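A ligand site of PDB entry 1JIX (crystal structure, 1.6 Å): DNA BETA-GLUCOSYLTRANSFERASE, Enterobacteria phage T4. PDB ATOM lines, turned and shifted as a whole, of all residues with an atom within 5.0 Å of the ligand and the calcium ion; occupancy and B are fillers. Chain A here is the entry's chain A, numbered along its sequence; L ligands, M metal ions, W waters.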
ATOM      1  N   VAL A  18      -0.034  25.509   2.906  1.00  0.00           N
ATOM      2  CA  VAL A  18       1.112  25.452   2.003  1.00  0.00           C
ATOM      3  C   VAL A  18       2.493  25.668   2.615  1.00  0.00           C
ATOM      4  O   VAL A  18       3.394  24.846   2.413  1.00  0.00           O
ATOM      5  CB  VAL A  18       0.928  26.437   0.835  1.00  0.00           C
ATOM      6  CG1 VAL A  18       2.124  26.368  -0.103  1.00  0.00           C
ATOM      7  CG2 VAL A  18      -0.347  26.118   0.077  1.00  0.00           C
ATOM      8  N   GLU A  22       5.425  22.864   2.502  1.00  0.00           N
ATOM      9  CA  GLU A  22       6.757  23.074   1.954  1.00  0.00           C
ATOM     10  C   GLU A  22       7.847  22.796   2.969  1.00  0.00           C
ATOM     11  O   GLU A  22       8.880  22.208   2.641  1.00  0.00           O
ATOM     12  CB  GLU A  22       6.869  24.498   1.426  1.00  0.00           C
ATOM     13  CG  GLU A  22       5.863  24.801   0.342  1.00  0.00           C
ATOM     14  CD  GLU A  22       5.881  26.252  -0.080  1.00  0.00           C
ATOM     15  OE1 GLU A  22       5.658  27.122   0.794  1.00  0.00           O
ATOM     16  OE2 GLU A  22       6.097  26.517  -1.279  1.00  0.00           O
ATOM     17  N   ASP A 100      11.155  32.378  -3.144  1.00  0.00           N
ATOM     18  CA  ASP A 100      10.201  33.354  -3.660  1.00  0.00           C
ATOM     19  C   ASP A 100      10.855  34.729  -3.635  1.00  0.00           C
ATOM     20  O   ASP A 100      11.236  35.234  -2.583  1.00  0.00           O
ATOM     21  CB  ASP A 100       8.934  33.350  -2.798  1.00  0.00           C
ATOM     22  CG  ASP A 100       7.797  34.164  -3.398  1.00  0.00           C
ATOM     23  OD1 ASP A 100       6.629  33.753  -3.250  1.00  0.00           O
ATOM     24  OD2 ASP A 100       8.074  35.229  -4.007  1.00  0.00           O
ATOM     25  N   ARG A 102       9.774  37.608  -3.674  1.00  0.00           N
ATOM     26  CA  ARG A 102       9.143  38.602  -2.807  1.00  0.00           C
ATOM     27  C   ARG A 102       9.440  38.403  -1.325  1.00  0.00           C
ATOM     28  O   ARG A 102       9.046  39.231  -0.511  1.00  0.00           O
ATOM     29  CB  ARG A 102       7.632  38.562  -2.963  1.00  0.00           C
ATOM     30  CG  ARG A 102       7.089  38.668  -4.381  1.00  0.00           C
ATOM     31  CD  ARG A 102       5.613  38.335  -4.335  1.00  0.00           C
ATOM     32  NE  ARG A 102       5.407  37.067  -3.615  1.00  0.00           N
ATOM     33  CZ  ARG A 102       4.245  36.645  -3.135  1.00  0.00           C
ATOM     34  NH1 ARG A 102       4.179  35.484  -2.502  1.00  0.00           N
ATOM     35  NH2 ARG A 102       3.153  37.387  -3.273  1.00  0.00           N
ATOM     36  N   TYR A 186      -4.621  26.489 -13.986  1.00  0.00           N
ATOM     37  CA  TYR A 186      -3.504  27.181 -13.341  1.00  0.00           C
ATOM     38  C   TYR A 186      -3.854  27.323 -11.884  1.00  0.00           C
ATOM     39  O   TYR A 186      -4.942  27.809 -11.541  1.00  0.00           O
ATOM     40  CB  TYR A 186      -3.281  28.563 -13.970  1.00  0.00           C
ATOM     41  CG  TYR A 186      -2.221  29.409 -13.271  1.00  0.00           C
ATOM     42  CD1 TYR A 186      -2.549  30.250 -12.216  1.00  0.00           C
ATOM     43  CD2 TYR A 186      -0.890  29.371 -13.692  1.00  0.00           C
ATOM     44  CE1 TYR A 186      -1.573  31.039 -11.586  1.00  0.00           C
ATOM     45  CE2 TYR A 186       0.098  30.154 -13.079  1.00  0.00           C
ATOM     46  CZ  TYR A 186      -0.262  30.990 -12.028  1.00  0.00           C
ATOM     47  OH  TYR A 186       0.709  31.764 -11.424  1.00  0.00           O
ATOM     48  N   GLY A 187      -2.941  26.907 -11.013  1.00  0.00           N
ATOM     49  CA  GLY A 187      -3.184  27.021  -9.590  1.00  0.00           C
ATOM     50  C   GLY A 187      -2.176  27.939  -8.937  1.00  0.00           C
ATOM     51  O   GLY A 187      -0.976  27.804  -9.176  1.00  0.00           O
ATOM     52  N   GLY A 188      -2.658  28.868  -8.124  1.00  0.00           N
ATOM     53  CA  GLY A 188      -1.759  29.790  -7.453  1.00  0.00           C
ATOM     54  C   GLY A 188      -2.481  30.938  -6.802  1.00  0.00           C
ATOM     55  O   GLY A 188      -3.712  30.999  -6.786  1.00  0.00           O
ATOM     56  N   SER A 189      -1.715  31.877  -6.252  1.00  0.00           N
ATOM     57  CA  SER A 189      -2.294  33.038  -5.602  1.00  0.00           C
ATOM     58  C   SER A 189      -2.181  34.238  -6.528  1.00  0.00           C
ATOM     59  O   SER A 189      -1.606  34.149  -7.612  1.00  0.00           O
ATOM     60  CB  SER A 189      -1.572  33.346  -4.296  1.00  0.00           C
ATOM     61  OG  SER A 189      -0.338  33.993  -4.566  1.00  0.00           O
ATOM     62  N   ARG A 191      -0.456  36.758  -5.908  1.00  0.00           N
ATOM     63  CA  ARG A 191       0.918  37.265  -5.762  1.00  0.00           C
ATOM     64  C   ARG A 191       0.983  38.788  -5.754  1.00  0.00           C
ATOM     65  O   ARG A 191       1.887  39.391  -6.322  1.00  0.00           O
ATOM     66  CB  ARG A 191       1.817  36.708  -6.885  1.00  0.00           C
ATOM     67  CG  ARG A 191       2.017  35.195  -6.818  1.00  0.00           C
ATOM     68  CD  ARG A 191       3.073  34.722  -7.803  1.00  0.00           C
ATOM     69  NE  ARG A 191       4.362  35.371  -7.585  1.00  0.00           N
ATOM     70  CZ  ARG A 191       5.194  35.089  -6.597  1.00  0.00           C
ATOM     71  NH1 ARG A 191       4.882  34.147  -5.709  1.00  0.00           N
ATOM     72  NH2 ARG A 191       6.330  35.769  -6.475  1.00  0.00           N
ATOM     73  N   ARG A 195       2.042  39.390 -11.179  1.00  0.00           N
ATOM     74  CA  ARG A 195       1.980  38.584 -12.401  1.00  0.00           C
ATOM     75  C   ARG A 195       0.640  38.793 -13.107  1.00  0.00           C
ATOM     76  O   ARG A 195       0.240  37.981 -13.938  1.00  0.00           O
ATOM     77  CB  ARG A 195       2.151  37.122 -11.997  1.00  0.00           C
ATOM     78  CG  ARG A 195       2.416  36.158 -13.120  1.00  0.00           C
ATOM     79  CD  ARG A 195       2.623  34.759 -12.536  1.00  0.00           C
ATOM     80  NE  ARG A 195       3.763  34.710 -11.630  1.00  0.00           N
ATOM     81  CZ  ARG A 195       4.145  33.611 -10.966  1.00  0.00           C
ATOM     82  NH1 ARG A 195       3.446  32.486 -11.106  1.00  0.00           N
ATOM     83  NH2 ARG A 195       5.221  33.634 -10.199  1.00  0.00           N
ATOM     84  N   PHE A 213      -7.333  27.798  -9.897  1.00  0.00           N
ATOM     85  CA  PHE A 213      -7.562  27.394  -8.513  1.00  0.00           C
ATOM     86  C   PHE A 213      -6.502  28.007  -7.608  1.00  0.00           C
ATOM     87  O   PHE A 213      -5.442  28.414  -8.069  1.00  0.00           O
ATOM     88  CB  PHE A 213      -7.593  25.853  -8.355  1.00  0.00           C
ATOM     89  CG  PHE A 213      -6.279  25.148  -8.631  1.00  0.00           C
ATOM     90  CD1 PHE A 213      -5.898  24.840  -9.934  1.00  0.00           C
ATOM     91  CD2 PHE A 213      -5.486  24.707  -7.574  1.00  0.00           C
ATOM     92  CE1 PHE A 213      -4.734  24.087 -10.185  1.00  0.00           C
ATOM     93  CE2 PHE A 213      -4.322  23.965  -7.812  1.00  0.00           C
ATOM     94  CZ  PHE A 213      -3.949  23.653  -9.120  1.00  0.00           C
ATOM     95  N   GLY A 214      -6.812  28.115  -6.314  1.00  0.00           N
ATOM     96  CA  GLY A 214      -5.862  28.709  -5.394  1.00  0.00           C
ATOM     97  C   GLY A 214      -6.486  29.857  -4.622  1.00  0.00           C
ATOM     98  O   GLY A 214      -7.711  30.009  -4.612  1.00  0.00           O
ATOM     99  N   GLY A 236     -11.643  27.288  -5.059  1.00  0.00           N
ATOM    100  CA  GLY A 236     -10.830  27.411  -3.863  1.00  0.00           C
ATOM    101  C   GLY A 236      -9.451  26.762  -3.914  1.00  0.00           C
ATOM    102  O   GLY A 236      -9.084  26.101  -4.891  1.00  0.00           O
ATOM    103  N   LYS A 237      -8.686  26.964  -2.848  1.00  0.00           N
ATOM    104  CA  LYS A 237      -7.357  26.376  -2.791  1.00  0.00           C
ATOM    105  C   LYS A 237      -7.472  24.912  -2.359  1.00  0.00           C
ATOM    106  O   LYS A 237      -8.475  24.495  -1.785  1.00  0.00           O
ATOM    107  CB  LYS A 237      -6.478  27.152  -1.797  1.00  0.00           C
ATOM    108  CG  LYS A 237      -7.005  27.173  -0.381  1.00  0.00           C
ATOM    109  CD  LYS A 237      -6.095  28.003   0.525  1.00  0.00           C
ATOM    110  CE  LYS A 237      -6.584  28.010   1.954  1.00  0.00           C
ATOM    111  NZ  LYS A 237      -5.708  28.844   2.824  1.00  0.00           N
ATOM    112  N   ILE A 238      -6.445  24.132  -2.675  1.00  0.00           N
ATOM    113  CA  ILE A 238      -6.415  22.734  -2.302  1.00  0.00           C
ATOM    114  C   ILE A 238      -5.056  22.427  -1.702  1.00  0.00           C
ATOM    115  O   ILE A 238      -4.111  23.197  -1.872  1.00  0.00           O
ATOM    116  CB  ILE A 238      -6.637  21.818  -3.512  1.00  0.00           C
ATOM    117  CG1 ILE A 238      -5.507  22.014  -4.516  1.00  0.00           C
ATOM    118  CG2 ILE A 238      -7.984  22.127  -4.161  1.00  0.00           C
ATOM    119  CD1 ILE A 238      -5.492  20.964  -5.598  1.00  0.00           C
ATOM    120  N   PRO A 239      -4.935  21.295  -0.982  1.00  0.00           N
ATOM    121  CA  PRO A 239      -3.675  20.909  -0.351  1.00  0.00           C
ATOM    122  C   PRO A 239      -2.536  20.808  -1.363  1.00  0.00           C
ATOM    123  O   PRO A 239      -2.726  20.336  -2.481  1.00  0.00           O
ATOM    124  CB  PRO A 239      -3.997  19.556   0.272  1.00  0.00           C
ATOM    125  CG  PRO A 239      -5.453  19.672   0.594  1.00  0.00           C
ATOM    126  CD  PRO A 239      -5.999  20.321  -0.664  1.00  0.00           C
ATOM    127  N   MET A 240      -1.347  21.252  -0.967  1.00  0.00           N
ATOM    128  CA  MET A 240      -0.205  21.194  -1.861  1.00  0.00           C
ATOM    129  C   MET A 240       0.071  19.792  -2.406  1.00  0.00           C
ATOM    130  O   MET A 240       0.501  19.630  -3.544  1.00  0.00           O
ATOM    131  CB  MET A 240       1.040  21.728  -1.162  1.00  0.00           C
ATOM    132  CG  MET A 240       2.252  21.781  -2.063  1.00  0.00           C
ATOM    133  SD  MET A 240       3.696  22.366  -1.201  1.00  0.00           S
ATOM    134  CE  MET A 240       4.983  21.681  -2.205  1.00  0.00           C
ATOM    135  N   VAL A 243      -1.917  18.971  -5.722  1.00  0.00           N
ATOM    136  CA  VAL A 243      -1.779  19.834  -6.887  1.00  0.00           C
ATOM    137  C   VAL A 243      -1.608  19.143  -8.242  1.00  0.00           C
ATOM    138  O   VAL A 243      -2.272  19.530  -9.206  1.00  0.00           O
ATOM    139  CB  VAL A 243      -0.644  20.853  -6.670  1.00  0.00           C
ATOM    140  CG1 VAL A 243      -0.391  21.665  -7.935  1.00  0.00           C
ATOM    141  CG2 VAL A 243      -1.027  21.784  -5.526  1.00  0.00           C
ATOM    142  N   ILE A 256       3.735  30.273 -16.077  1.00  0.00           N
ATOM    143  CA  ILE A 256       4.098  31.677 -16.187  1.00  0.00           C
ATOM    144  C   ILE A 256       4.819  32.017 -14.887  1.00  0.00           C
ATOM    145  O   ILE A 256       4.780  31.244 -13.930  1.00  0.00           O
ATOM    146  CB  ILE A 256       2.861  32.605 -16.328  1.00  0.00           C
ATOM    147  CG1 ILE A 256       1.786  32.202 -15.320  1.00  0.00           C
ATOM    148  CG2 ILE A 256       2.355  32.583 -17.760  1.00  0.00           C
ATOM    149  CD1 ILE A 256       0.638  33.209 -15.233  1.00  0.00           C
ATOM    150  N   TYR A 261      11.498  36.141 -12.699  1.00  0.00           N
ATOM    151  CA  TYR A 261      11.630  34.679 -12.720  1.00  0.00           C
ATOM    152  C   TYR A 261      12.048  34.217 -14.108  1.00  0.00           C
ATOM    153  O   TYR A 261      12.674  33.165 -14.267  1.00  0.00           O
ATOM    154  CB  TYR A 261      10.291  34.008 -12.367  1.00  0.00           C
ATOM    155  CG  TYR A 261       9.971  33.945 -10.884  1.00  0.00           C
ATOM    156  CD1 TYR A 261      10.819  34.524  -9.945  1.00  0.00           C
ATOM    157  CD2 TYR A 261       8.819  33.315 -10.431  1.00  0.00           C
ATOM    158  CE1 TYR A 261      10.527  34.478  -8.579  1.00  0.00           C
ATOM    159  CE2 TYR A 261       8.511  33.260  -9.074  1.00  0.00           C
ATOM    160  CZ  TYR A 261       9.367  33.842  -8.152  1.00  0.00           C
ATOM    161  OH  TYR A 261       9.087  33.800  -6.814  1.00  0.00           O
ATOM    162  N   THR A 267      10.335  27.106 -11.140  1.00  0.00           N
ATOM    163  CA  THR A 267       9.452  26.983  -9.993  1.00  0.00           C
ATOM    164  C   THR A 267       8.820  25.610  -9.777  1.00  0.00           C
ATOM    165  O   THR A 267       8.805  24.759 -10.665  1.00  0.00           O
ATOM    166  CB  THR A 267       8.319  28.008 -10.095  1.00  0.00           C
ATOM    167  OG1 THR A 267       7.713  27.902 -11.396  1.00  0.00           O
ATOM    168  CG2 THR A 267       8.874  29.421  -9.942  1.00  0.00           C
ATOM    169  N   LEU A 268       8.286  25.426  -8.572  1.00  0.00           N
ATOM    170  CA  LEU A 268       7.638  24.167  -8.202  1.00  0.00           C
ATOM    171  C   LEU A 268       6.568  23.764  -9.224  1.00  0.00           C
ATOM    172  O   LEU A 268       6.426  22.575  -9.535  1.00  0.00           O
ATOM    173  CB  LEU A 268       6.993  24.317  -6.830  1.00  0.00           C
ATOM    174  CG  LEU A 268       7.320  23.309  -5.724  1.00  0.00           C
ATOM    175  CD1 LEU A 268       6.287  23.455  -4.625  1.00  0.00           C
ATOM    176  CD2 LEU A 268       7.319  21.895  -6.272  1.00  0.00           C
ATOM    177  N   ARG A 269       5.823  24.729  -9.748  1.00  0.00           N
ATOM    178  CA  ARG A 269       4.776  24.408 -10.704  1.00  0.00           C
ATOM    179  C   ARG A 269       5.301  23.761 -11.973  1.00  0.00           C
ATOM    180  O   ARG A 269       4.573  23.023 -12.629  1.00  0.00           O
ATOM    181  CB  ARG A 269       3.929  25.645 -11.066  1.00  0.00           C
ATOM    182  CG  ARG A 269       4.607  26.651 -11.981  1.00  0.00           C
ATOM    183  CD  ARG A 269       3.603  27.705 -12.453  1.00  0.00           C
ATOM    184  NE  ARG A 269       3.057  28.477 -11.340  1.00  0.00           N
ATOM    185  CZ  ARG A 269       1.856  28.275 -10.787  1.00  0.00           C
ATOM    186  NH1 ARG A 269       1.044  27.341 -11.257  1.00  0.00           N
ATOM    187  NH2 ARG A 269       1.486  29.027  -9.754  1.00  0.00           N
ATOM    188  N   GLU A 272       5.355  20.241 -10.831  1.00  0.00           N
ATOM    189  CA  GLU A 272       4.002  19.771 -10.530  1.00  0.00           C
ATOM    190  C   GLU A 272       3.211  19.576 -11.817  1.00  0.00           C
ATOM    191  O   GLU A 272       2.355  18.689 -11.912  1.00  0.00           O
ATOM    192  CB  GLU A 272       3.248  20.784  -9.660  1.00  0.00           C
ATOM    193  CG  GLU A 272       3.856  20.974  -8.280  1.00  0.00           C
ATOM    194  CD  GLU A 272       3.236  22.132  -7.549  1.00  0.00           C
ATOM    195  OE1 GLU A 272       2.857  23.120  -8.228  1.00  0.00           O
ATOM    196  OE2 GLU A 272       3.144  22.086  -6.304  1.00  0.00           O
HETATM  197  N1  LIG L   1      -0.616  25.706  -4.512  1.00  0.00           N
HETATM  198  C1  LIG L   1      -1.242  24.856  -3.638  1.00  0.00           C
HETATM  199  N2  LIG L   1      -2.618  24.854  -3.685  1.00  0.00           N
HETATM  200  C2  LIG L   1      -3.412  25.621  -4.516  1.00  0.00           C
HETATM  201  C3  LIG L   1      -2.688  26.472  -5.412  1.00  0.00           C
HETATM  202  C4  LIG L   1      -1.357  26.484  -5.384  1.00  0.00           C
HETATM  203  O1  LIG L   1      -0.626  24.133  -2.868  1.00  0.00           O
HETATM  204  O2  LIG L   1      -4.635  25.569  -4.403  1.00  0.00           O
HETATM  205  C5  LIG L   1       0.844  25.770  -4.473  1.00  0.00           C
HETATM  206  C6  LIG L   1       1.549  24.870  -5.480  1.00  0.00           C
HETATM  207  O3  LIG L   1       2.699  24.305  -4.891  1.00  0.00           O
HETATM  208  C7  LIG L   1       1.913  25.857  -6.582  1.00  0.00           C
HETATM  209  C8  LIG L   1       2.213  27.119  -5.792  1.00  0.00           C
HETATM  210  O4  LIG L   1       1.245  27.106  -4.709  1.00  0.00           O
HETATM  211  O5  LIG L   1       3.078  25.443  -7.288  1.00  0.00           O
HETATM  212  C9  LIG L   1       2.078  28.408  -6.571  1.00  0.00           C
HETATM  213  O6  LIG L   1       2.625  29.486  -5.832  1.00  0.00           O
HETATM  214  P1  LIG L   1       2.506  30.986  -6.373  1.00  0.00           P
HETATM  215  O7  LIG L   1       1.058  31.285  -6.582  1.00  0.00           O
HETATM  216  O8  LIG L   1       3.300  31.859  -5.479  1.00  0.00           O
HETATM  217  O9  LIG L   1       3.177  30.910  -7.821  1.00  0.00           O
HETATM  218  P2  LIG L   1       4.687  30.624  -8.267  1.00  0.00           P
HETATM  219  O10 LIG L   1       5.331  31.941  -8.023  1.00  0.00           O
HETATM  220  O11 LIG L   1       4.472  30.265  -9.688  1.00  0.00           O
HETATM  221  O12 LIG L   1       5.106  29.524  -7.366  1.00  0.00           O
HETATM  222 CA    CA M   1       6.229  28.543  -5.196  1.00  0.00          CA
HETATM  223  O   HOH W   1      -0.255  29.723  -4.090  1.00  0.00           O
HETATM  224  O   HOH W   2       0.229  32.562  -8.964  1.00  0.00           O
HETATM  225  O   HOH W   3       1.851  32.909  -3.409  1.00  0.00           O
HETATM  226  O   HOH W   4       7.307  28.558  -2.596  1.00  0.00           O
HETATM  227  O   HOH W   5       4.149  26.035  -3.200  1.00  0.00           O
HETATM  228  O   HOH W   6       8.733  27.289  -6.399  1.00  0.00           O
HETATM  229  O   HOH W   7       7.295  31.903  -6.187  1.00  0.00           O
HETATM  230  O   HOH W   8       5.204  26.911  -8.297  1.00  0.00           O
HETATM  231  O   HOH W   9       3.058  28.646  -2.268  1.00  0.00           O
HETATM  232  O   HOH W  10       5.902  30.620  -4.129  1.00  0.00           O
HETATM  233  O   HOH W  11       6.227  30.060 -11.824  1.00  0.00           O
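The guanidinium group of Arg 269 lies within salt-bridge range of an oxygen (O11) of the ligand. An oxygen (O5) of the ligand is in hydrogen-bond range of the side-chain carboxylate (OE1) of Glu 272 (2.5 Å). The backbone NH of Ser 189 lies within hydrogen-bond range of an oxygen (O7) of the ligand (2.9 Å). The backbone NH (N) of Ile 238 sits at hydrogen-bond distance from an oxygen (O2) of the ligand, at 2.9 Å. The guanidinium group of Arg 191 is in salt-bridge range of an oxygen (O8) of the ligand, 2.8 Å away. The backbone carbonyl oxygen of Ile 238 lies within hydrogen-bond range of a nitrogen (N2) of the ligand (2.9 Å). O10 of the ligand is in salt-bridge range of NH2 of Arg 195 (2.8 Å).
OD2 of Asp 100 lies within hydrogen-bond range of OH of Tyr 261 (3.3 Å). The guanidinium group (NH1) of Arg 195 is in hydrogen-bond range of the backbone carbonyl oxygen (O) of Ile 256 (3.4 Å). OD1 of Asp 100 is in salt-bridge range of NH1 of Arg 191 (3.0 Å). N of Gly 214 lies within hydrogen-bond range of O of Gly 236 (3.4 Å). The backbone carbonyl oxygen (O) of Phe 213 is in hydrogen-bond range of the backbone NH (N) of Gly 188. The side-chain hydroxyl (OH) of Tyr 186 lies within hydrogen-bond range of the guanidinium group (NH2) of Arg 269 (3.3 Å). The backbone NH of Arg 191 is in hydrogen-bond range of the side-chain hydroxyl of Ser 189, 3.1 Å away. The side-chain hydroxyl (OH) of Tyr 186 is in hydrogen-bond range of the guanidinium group (NH1) of Arg 195.
Val 18 touches the ligand. Gly 187 touches the ligand (C to C3, 3.9 Å). Gly 188 touches the ligand (CA to O7, 3.3 Å). CD2 of Phe 213 touches O2 of the ligand (3.4 Å). Gly 214 touches the ligand (CA to O2, 3.5 Å). CA of Lys 237 touches O2 of the ligand (3.3 Å). Met 240 touches the ligand (CA to O1, 3.1 Å). Val 243 touches the ligand. Tyr 261 touches the ligand. Leu 268 touches the ligand. Hydrophobic or aromatic side chains that line the ligand: Val 18, Phe 213, Ile 238, Met 240, Val 243, Tyr 261 and Leu 268. 16 residues have an atom within 4 Å of the ligand: Val 18, Gly 187, Gly 188, Ser 189, Arg 191, Arg 195, Phe 213, Gly 214, Lys 237, Ile 238, Met 240, Val 243, Tyr 261, Leu 268, Arg 269 and Glu 272. The nearest printed residue that does not touch the ligand is Pro 239 (4.1 Å).
No residue comes within 4 Å of the calcium ion.
The calcium ion is bound by water W10 (2.4 Å), an oxygen (O12) of the ligand (2.6 Å) and water W4 (2.8 Å). Slightly farther from the calcium ion lies water W6 (3.0 Å).
Water W10 bridges an oxygen (O8) of the ligand (3.2 Å) and the side-chain carboxylate (OD1) of Asp 100 (3.3 Å). Water W7 lies within hydrogen-bond range of the side-chain hydroxyl of Tyr 261, an oxygen (O10) of the ligand and the guanidinium group of Arg 191. Water W3 lies within hydrogen-bond range of OG of Ser 189 (2.7 Å) and O8 of the ligand (2.7 Å). Water W8 lies within hydrogen-bond range of the backbone NH of Arg 269 (2.7 Å), an oxygen (O5) of the ligand (2.8 Å) and the backbone NH of Leu 268 (3.4 Å). Water W5 bridges OE2 of Glu 22 (2.8 Å) and O3 of the ligand (2.8 Å). Water W2 lies within hydrogen-bond range of OH of Tyr 186, O of Ser 189 and O7 of the ligand.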
